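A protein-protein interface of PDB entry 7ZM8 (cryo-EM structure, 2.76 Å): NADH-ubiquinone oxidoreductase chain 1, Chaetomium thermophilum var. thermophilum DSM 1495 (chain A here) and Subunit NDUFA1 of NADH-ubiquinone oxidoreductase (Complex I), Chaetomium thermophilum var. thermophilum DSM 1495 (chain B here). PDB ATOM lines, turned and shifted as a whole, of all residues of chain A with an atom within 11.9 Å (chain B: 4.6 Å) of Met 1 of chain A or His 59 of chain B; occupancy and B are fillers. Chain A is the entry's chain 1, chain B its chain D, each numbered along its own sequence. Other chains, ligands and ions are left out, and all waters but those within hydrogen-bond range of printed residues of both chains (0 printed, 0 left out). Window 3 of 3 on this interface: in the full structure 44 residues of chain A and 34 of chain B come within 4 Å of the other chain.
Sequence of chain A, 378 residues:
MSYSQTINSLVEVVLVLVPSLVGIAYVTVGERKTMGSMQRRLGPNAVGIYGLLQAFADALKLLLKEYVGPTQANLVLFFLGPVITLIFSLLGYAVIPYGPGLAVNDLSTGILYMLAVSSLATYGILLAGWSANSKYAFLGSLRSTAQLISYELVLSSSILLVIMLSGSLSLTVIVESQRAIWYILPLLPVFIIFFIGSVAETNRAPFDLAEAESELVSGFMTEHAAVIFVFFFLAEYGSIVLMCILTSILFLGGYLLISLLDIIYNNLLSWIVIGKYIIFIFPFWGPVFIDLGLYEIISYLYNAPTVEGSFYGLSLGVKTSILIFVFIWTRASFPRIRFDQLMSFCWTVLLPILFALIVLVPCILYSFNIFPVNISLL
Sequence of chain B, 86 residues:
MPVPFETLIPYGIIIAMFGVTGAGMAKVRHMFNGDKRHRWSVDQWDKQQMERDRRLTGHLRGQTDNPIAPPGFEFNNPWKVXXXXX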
ATOM      1  N   MET A   1      22.762  15.534  -3.725  1.00  0.00           N
ATOM      2  CA  MET A   1      23.096  14.171  -3.335  1.00  0.00           C
ATOM      3  C   MET A   1      22.758  13.186  -4.445  1.00  0.00           C
ATOM      4  O   MET A   1      22.106  13.543  -5.421  1.00  0.00           O
ATOM      5  CB  MET A   1      22.380  13.795  -2.051  1.00  0.00           C
ATOM      6  CG  MET A   1      22.859  14.584  -0.849  1.00  0.00           C
ATOM      7  SD  MET A   1      24.548  14.164  -0.359  1.00  0.00           S
ATOM      8  CE  MET A   1      25.108  15.717   0.326  1.00  0.00           C
ATOM      9  N   SER A   2      23.205  11.942  -4.293  1.00  0.00           N
ATOM     10  CA  SER A   2      23.193  10.991  -5.397  1.00  0.00           C
ATOM     11  C   SER A   2      21.915  10.163  -5.446  1.00  0.00           C
ATOM     12  O   SER A   2      21.338   9.978  -6.521  1.00  0.00           O
ATOM     13  CB  SER A   2      24.414  10.076  -5.304  1.00  0.00           C
ATOM     14  OG  SER A   2      25.603  10.837  -5.225  1.00  0.00           O
ATOM     15  N   TYR A   3      21.498   9.670  -4.282  1.00  0.00           N
ATOM     16  CA  TYR A   3      20.253   8.885  -4.184  1.00  0.00           C
ATOM     17  C   TYR A   3      19.349   9.528  -3.136  1.00  0.00           C
ATOM     18  O   TYR A   3      19.730  10.552  -2.591  1.00  0.00           O
ATOM     19  CB  TYR A   3      20.552   7.396  -3.989  1.00  0.00           C
ATOM     20  CG  TYR A   3      21.315   6.990  -2.755  1.00  0.00           C
ATOM     21  CD1 TYR A   3      20.660   6.739  -1.563  1.00  0.00           C
ATOM     22  CD2 TYR A   3      22.684   6.794  -2.792  1.00  0.00           C
ATOM     23  CE1 TYR A   3      21.347   6.352  -0.428  1.00  0.00           C
ATOM     24  CE2 TYR A   3      23.386   6.397  -1.668  1.00  0.00           C
ATOM     25  CZ  TYR A   3      22.716   6.181  -0.479  1.00  0.00           C
ATOM     26  OH  TYR A   3      23.390   5.795   0.640  1.00  0.00           O
ATOM     27  N   SER A   4      18.167   8.943  -2.915  1.00  0.00           N
ATOM     28  CA  SER A   4      17.177   9.502  -1.969  1.00  0.00           C
ATOM     29  C   SER A   4      17.669   9.476  -0.527  1.00  0.00           C
ATOM     30  O   SER A   4      18.309   8.484  -0.136  1.00  0.00           O
ATOM     31  CB  SER A   4      15.896   8.781  -2.108  1.00  0.00           C
ATOM     32  OG  SER A   4      16.122   7.390  -2.232  1.00  0.00           O
ATOM     33  N   GLN A   5      17.348  10.535   0.229  1.00  0.00           N
ATOM     34  CA  GLN A   5      17.751  10.649   1.646  1.00  0.00           C
ATOM     35  C   GLN A   5      17.076   9.558   2.465  1.00  0.00           C
ATOM     36  O   GLN A   5      17.712   9.028   3.344  1.00  0.00           O
ATOM     37  CB  GLN A   5      17.349  12.032   2.152  1.00  0.00           C
ATOM     38  CG  GLN A   5      18.490  12.788   2.809  1.00  0.00           C
ATOM     39  CD  GLN A   5      18.153  14.249   2.951  1.00  0.00           C
ATOM     40  OE1 GLN A   5      17.025  14.668   2.707  1.00  0.00           O
ATOM     41  NE2 GLN A   5      19.138  15.039   3.347  1.00  0.00           N
ATOM     42  N   THR A   6      15.823   9.253   2.178  1.00  0.00           N
ATOM     43  CA  THR A   6      15.068   8.262   2.973  1.00  0.00           C
ATOM     44  C   THR A   6      15.762   6.913   2.888  1.00  0.00           C
ATOM     45  O   THR A   6      15.869   6.267   3.934  1.00  0.00           O
ATOM     46  CB  THR A   6      13.657   8.086   2.412  1.00  0.00           C
ATOM     47  OG1 THR A   6      13.039   9.371   2.350  1.00  0.00           O
ATOM     48  CG2 THR A   6      12.798   7.147   3.229  1.00  0.00           C
ATOM     49  N   ILE A   7      16.211   6.506   1.703  1.00  0.00           N
ATOM     50  CA  ILE A   7      16.985   5.244   1.588  1.00  0.00           C
ATOM     51  C   ILE A   7      18.258   5.399   2.416  1.00  0.00           C
ATOM     52  O   ILE A   7      18.533   4.511   3.215  1.00  0.00           O
ATOM     53  CB  ILE A   7      17.266   4.893   0.119  1.00  0.00           C
ATOM     54  CG1 ILE A   7      15.972   4.638  -0.656  1.00  0.00           C
ATOM     55  CG2 ILE A   7      18.228   3.722   0.007  1.00  0.00           C
ATOM     56  CD1 ILE A   7      15.175   3.462  -0.148  1.00  0.00           C
ATOM     57  N   ASN A   8      19.017   6.477   2.223  1.00  0.00           N
ATOM     58  CA  ASN A   8      20.268   6.699   2.981  1.00  0.00           C
ATOM     59  C   ASN A   8      19.968   6.513   4.465  1.00  0.00           C
ATOM     60  O   ASN A   8      20.736   5.830   5.141  1.00  0.00           O
ATOM     61  CB  ASN A   8      20.864   8.085   2.723  1.00  0.00           C
ATOM     62  CG  ASN A   8      22.228   8.291   3.347  1.00  0.00           C
ATOM     63  OD1 ASN A   8      23.185   7.596   3.021  1.00  0.00           O
ATOM     64  ND2 ASN A   8      22.331   9.265   4.232  1.00  0.00           N
ATOM     65  N   SER A   9      18.933   7.173   4.960  1.00  0.00           N
ATOM     66  CA  SER A   9      18.599   7.126   6.402  1.00  0.00           C
ATOM     67  C   SER A   9      18.352   5.686   6.840  1.00  0.00           C
ATOM     68  O   SER A   9      18.926   5.289   7.850  1.00  0.00           O
ATOM     69  CB  SER A   9      17.416   7.999   6.664  1.00  0.00           C
ATOM     70  OG  SER A   9      17.690   9.340   6.295  1.00  0.00           O
ATOM     71  N   GLU A  12      21.585   3.479   6.929  1.00  0.00           N
ATOM     72  CA  GLU A  12      22.415   3.802   8.111  1.00  0.00           C
ATOM     73  C   GLU A  12      21.782   3.283   9.401  1.00  0.00           C
ATOM     74  O   GLU A  12      22.504   2.719  10.235  1.00  0.00           O
ATOM     75  CB  GLU A  12      22.739   5.289   8.141  1.00  0.00           C
ATOM     76  CG  GLU A  12      23.428   5.753   6.874  1.00  0.00           C
ATOM     77  CD  GLU A  12      24.064   7.126   6.951  1.00  0.00           C
ATOM     78  OE1 GLU A  12      23.319   8.117   7.002  1.00  0.00           O
ATOM     79  OE2 GLU A  12      25.306   7.192   6.965  1.00  0.00           O
ATOM     80  N   GLY A 101      32.387  11.785  11.822  1.00  0.00           N
ATOM     81  CA  GLY A 101      31.027  12.130  11.486  1.00  0.00           C
ATOM     82  C   GLY A 101      30.159  10.982  11.043  1.00  0.00           C
ATOM     83  O   GLY A 101      29.057  11.221  10.543  1.00  0.00           O
ATOM     84  N   PHE B  32      26.590   8.138  -1.291  1.00  0.00           N
ATOM     85  CA  PHE B  32      25.570   9.204  -1.104  1.00  0.00           C
ATOM     86  C   PHE B  32      26.155  10.550  -1.511  1.00  0.00           C
ATOM     87  O   PHE B  32      25.404  11.398  -2.004  1.00  0.00           O
ATOM     88  CB  PHE B  32      25.031   9.232   0.325  1.00  0.00           C
ATOM     89  CG  PHE B  32      23.784  10.052   0.524  1.00  0.00           C
ATOM     90  CD1 PHE B  32      22.634   9.774  -0.190  1.00  0.00           C
ATOM     91  CD2 PHE B  32      23.757  11.092   1.440  1.00  0.00           C
ATOM     92  CE1 PHE B  32      21.483  10.517   0.006  1.00  0.00           C
ATOM     93  CE2 PHE B  32      22.604  11.835   1.632  1.00  0.00           C
ATOM     94  CZ  PHE B  32      21.469  11.543   0.915  1.00  0.00           C
ATOM     95  N   ASN B  33      27.449  10.733  -1.285  1.00  0.00           N
ATOM     96  CA  ASN B  33      28.106  12.039  -1.510  1.00  0.00           C
ATOM     97  C   ASN B  33      28.718  12.104  -2.903  1.00  0.00           C
ATOM     98  O   ASN B  33      29.406  13.058  -3.174  1.00  0.00           O
ATOM     99  CB  ASN B  33      29.018  12.376  -0.336  1.00  0.00           C
ATOM    100  CG  ASN B  33      28.249  12.806   0.890  1.00  0.00           C
ATOM    101  OD1 ASN B  33      27.881  13.966   1.009  1.00  0.00           O
ATOM    102  ND2 ASN B  33      28.000  11.886   1.802  1.00  0.00           N
ATOM    103  N   GLY B  34      28.455  11.127  -3.754  1.00  0.00           N
ATOM    104  CA  GLY B  34      28.899  11.196  -5.150  1.00  0.00           C
ATOM    105  C   GLY B  34      30.237  10.546  -5.319  1.00  0.00           C
ATOM    106  O   GLY B  34      31.114  11.180  -5.934  1.00  0.00           O
ATOM    107  N   ASP B  53      27.491  25.136  -4.174  1.00  0.00           N
ATOM    108  CA  ASP B  53      27.950  24.095  -5.088  1.00  0.00           C
ATOM    109  C   ASP B  53      26.796  23.553  -5.915  1.00  0.00           C
ATOM    110  O   ASP B  53      26.965  23.234  -7.095  1.00  0.00           O
ATOM    111  CB  ASP B  53      28.607  22.959  -4.307  1.00  0.00           C
ATOM    112  CG  ASP B  53      29.912  23.364  -3.674  1.00  0.00           C
ATOM    113  OD1 ASP B  53      30.589  24.254  -4.220  1.00  0.00           O
ATOM    114  OD2 ASP B  53      30.280  22.761  -2.644  1.00  0.00           O
ATOM    115  N   ARG B  54      25.613  23.423  -5.318  1.00  0.00           N
ATOM    116  CA  ARG B  54      24.399  23.004  -6.067  1.00  0.00           C
ATOM    117  C   ARG B  54      23.973  24.102  -7.038  1.00  0.00           C
ATOM    118  O   ARG B  54      23.375  23.769  -8.067  1.00  0.00           O
ATOM    119  CB  ARG B  54      23.281  22.659  -5.079  1.00  0.00           C
ATOM    120  CG  ARG B  54      22.080  21.964  -5.701  1.00  0.00           C
ATOM    121  CD  ARG B  54      21.212  21.255  -4.683  1.00  0.00           C
ATOM    122  NE  ARG B  54      20.773  22.167  -3.640  1.00  0.00           N
ATOM    123  CZ  ARG B  54      19.992  21.830  -2.623  1.00  0.00           C
ATOM    124  NH1 ARG B  54      19.654  22.737  -1.724  1.00  0.00           N
ATOM    125  NH2 ARG B  54      19.554  20.591  -2.507  1.00  0.00           N
ATOM    126  N   THR B  57      26.713  23.552  -9.980  1.00  0.00           N
ATOM    127  CA  THR B  57      26.754  22.235 -10.603  1.00  0.00           C
ATOM    128  C   THR B  57      25.453  21.455 -10.527  1.00  0.00           C
ATOM    129  O   THR B  57      25.221  20.602 -11.381  1.00  0.00           O
ATOM    130  CB  THR B  57      27.863  21.374  -9.977  1.00  0.00           C
ATOM    131  OG1 THR B  57      27.426  20.887  -8.705  1.00  0.00           O
ATOM    132  CG2 THR B  57      29.148  22.171  -9.810  1.00  0.00           C
ATOM    133  N   GLY B  58      24.603  21.713  -9.541  1.00  0.00           N
ATOM    134  CA  GLY B  58      23.407  20.926  -9.328  1.00  0.00           C
ATOM    135  C   GLY B  58      23.519  19.901  -8.223  1.00  0.00           C
ATOM    136  O   GLY B  58      22.492  19.386  -7.774  1.00  0.00           O
ATOM    137  N   HIS B  59      24.731  19.610  -7.765  1.00  0.00           N
ATOM    138  CA  HIS B  59      25.001  18.648  -6.709  1.00  0.00           C
ATOM    139  C   HIS B  59      25.642  19.368  -5.535  1.00  0.00           C
ATOM    140  O   HIS B  59      26.540  20.189  -5.722  1.00  0.00           O
ATOM    141  CB  HIS B  59      25.920  17.537  -7.226  1.00  0.00           C
ATOM    142  CG  HIS B  59      26.121  16.404  -6.268  1.00  0.00           C
ATOM    143  ND1 HIS B  59      25.436  16.313  -5.077  1.00  0.00           N
ATOM    144  CD2 HIS B  59      26.915  15.309  -6.325  1.00  0.00           C
ATOM    145  CE1 HIS B  59      25.803  15.217  -4.440  1.00  0.00           C
ATOM    146  NE2 HIS B  59      26.700  14.590  -5.176  1.00  0.00           N
ATOM    147  N   LEU B  60      25.176  19.057  -4.322  1.00  0.00           N
ATOM    148  CA  LEU B  60      25.687  19.731  -3.133  1.00  0.00           C
ATOM    149  C   LEU B  60      27.176  19.492  -2.934  1.00  0.00           C
ATOM    150  O   LEU B  60      27.847  20.292  -2.277  1.00  0.00           O
ATOM    151  CB  LEU B  60      24.914  19.283  -1.893  1.00  0.00           C
ATOM    152  CG  LEU B  60      23.483  19.807  -1.757  1.00  0.00           C
ATOM    153  CD1 LEU B  60      22.658  18.927  -0.841  1.00  0.00           C
ATOM    154  CD2 LEU B  60      23.471  21.248  -1.276  1.00  0.00           C
ATOM    155  N   ARG B  61      27.715  18.410  -3.487  1.00  0.00           N
ATOM    156  CA  ARG B  61      29.139  18.135  -3.414  1.00  0.00           C
ATOM    157  C   ARG B  61      29.851  18.355  -4.742  1.00  0.00           C
ATOM    158  O   ARG B  61      31.037  18.034  -4.857  1.00  0.00           O
ATOM    159  CB  ARG B  61      29.382  16.708  -2.924  1.00  0.00           C
ATOM    160  CG  ARG B  61      28.675  16.368  -1.631  1.00  0.00           C
ATOM    161  CD  ARG B  61      29.267  17.108  -0.447  1.00  0.00           C
ATOM    162  NE  ARG B  61      30.725  17.100  -0.459  1.00  0.00           N
ATOM    163  CZ  ARG B  61      31.471  16.126   0.048  1.00  0.00           C
ATOM    164  NH1 ARG B  61      32.788  16.202  -0.009  1.00  0.00           N
ATOM    165  NH2 ARG B  61      30.902  15.078   0.614  1.00  0.00           N
ATOM    166  N   GLY B  62      29.164  18.894  -5.744  1.00  0.00           N
ATOM    167  CA  GLY B  62      29.804  19.130  -7.021  1.00  0.00           C
ATOM    168  C   GLY B  62      30.811  20.260  -6.956  1.00  0.00           C
ATOM    169  O   GLY B  62      30.657  21.222  -6.208  1.00  0.00           O
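N of Met 1 of chain A lies within hydrogen-bond range of ND1 of His 59 of chain B (3.1 Å). The backbone carbonyl oxygen (O) of Phe 32 of chain B lies close to the side-chain sulfur (SD) of Met 1 of chain A. N of Gly 34 of chain B sits at hydrogen-bond distance from OG of Ser 2 of chain A, at 3.2 Å. OD1 of Asn 33 of chain B sits close to SD of Met 1 of chain A, 3.6 Å away. The backbone NH (N) of Ser 2 of chain A lies within hydrogen-bond range of the backbone carbonyl oxygen (O) of Phe 32 of chain B (3.2 Å).
ND1 of His 59 of chain B lies close to N of Arg 61 of chain B. N of Arg 54 of chain B sits at hydrogen-bond distance from O of His 59 of chain B (3.4 Å). OD1 of Asn 8 of chain A sits at hydrogen-bond distance from OH of Tyr 3 of chain A (3.0 Å). ND2 of Asn 8 of chain A lies within hydrogen-bond range of OE1 of Glu 12 of chain A, 3.2 Å away. The guanidinium group (NH2) of Arg 61 of chain B lies within hydrogen-bond range of the side-chain amide oxygen (OD1) of Asn 33 of chain B, at 3.2 Å. N of His 59 of chain B sits at hydrogen-bond distance from OG1 of Thr 57 of chain B (3.1 Å).
His 59 of chain B touches Ser 2 of chain A (NE2 to OG, 3.9 Å). Phe 32 of chain B touches Tyr 3 of chain A. Phe 32 of chain B touches Ser 4 of chain A (CE1 to O, 3.8 Å). Gln 5 of chain A touches Phe 32 of chain B (CG to CZ, 3.7 Å). Asn 8 of chain A touches Phe 32 of chain B.
Met 1 of chain A touches three residues of chain B. Of the printed residues of chain A, Phe 32 of chain B touches Met 1, Ser 2, Tyr 3, Ser 4, Gln 5 and Asn 8. Of the printed residues of chain A, Asn 33 of chain B touches Met 1. Gly 34 of chain B touches one residue of chain A. No residue of chain A comes within 4 Å of Thr 57 of chain B. No residue of chain A comes within 4 Å of Gly 58 of chain B. No residue of chain A comes within 4 Å of Leu 60 of chain B. No residue of chain A comes within 4 Å of Arg 61 of chain B. Of the printed residues of chain B, Ser 2 of chain A touches Phe 32 (3.2 Å), Gly 34 (3.2 Å) and His 59 (3.9 Å). Of the printed residues of chain B, Tyr 3 of chain A touches Phe 32 (3.1 Å). Printed residues of chain B within 4 Å of Ser 4 of chain A: Phe 32 (3.8 Å). Printed residues of chain B within 4 Å of Gln 5 of chain A: Phe 32 (3.7 Å). Of the printed residues of chain B, Asn 8 of chain A touches Phe 32. The nearest residue of chain B that does not touch Met 1 of chain A is Arg 61 of chain B (4.1 Å). The nearest residue of chain A that does not touch His 59 of chain B is Tyr 3 of chain A (7.0 Å). The nearest printed residue of chain B that does not touch Asn 8 of chain A is Asn 33 of chain B (6.6 Å).
Of the 11 printed residues of chain B, 4 touch a printed residue of chain A. Hydrophobic or aromatic side chains of chain B that line the printed part of chain A: Phe 32 and His 59. Among the printed residues, 10 pairs touch across the chains.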
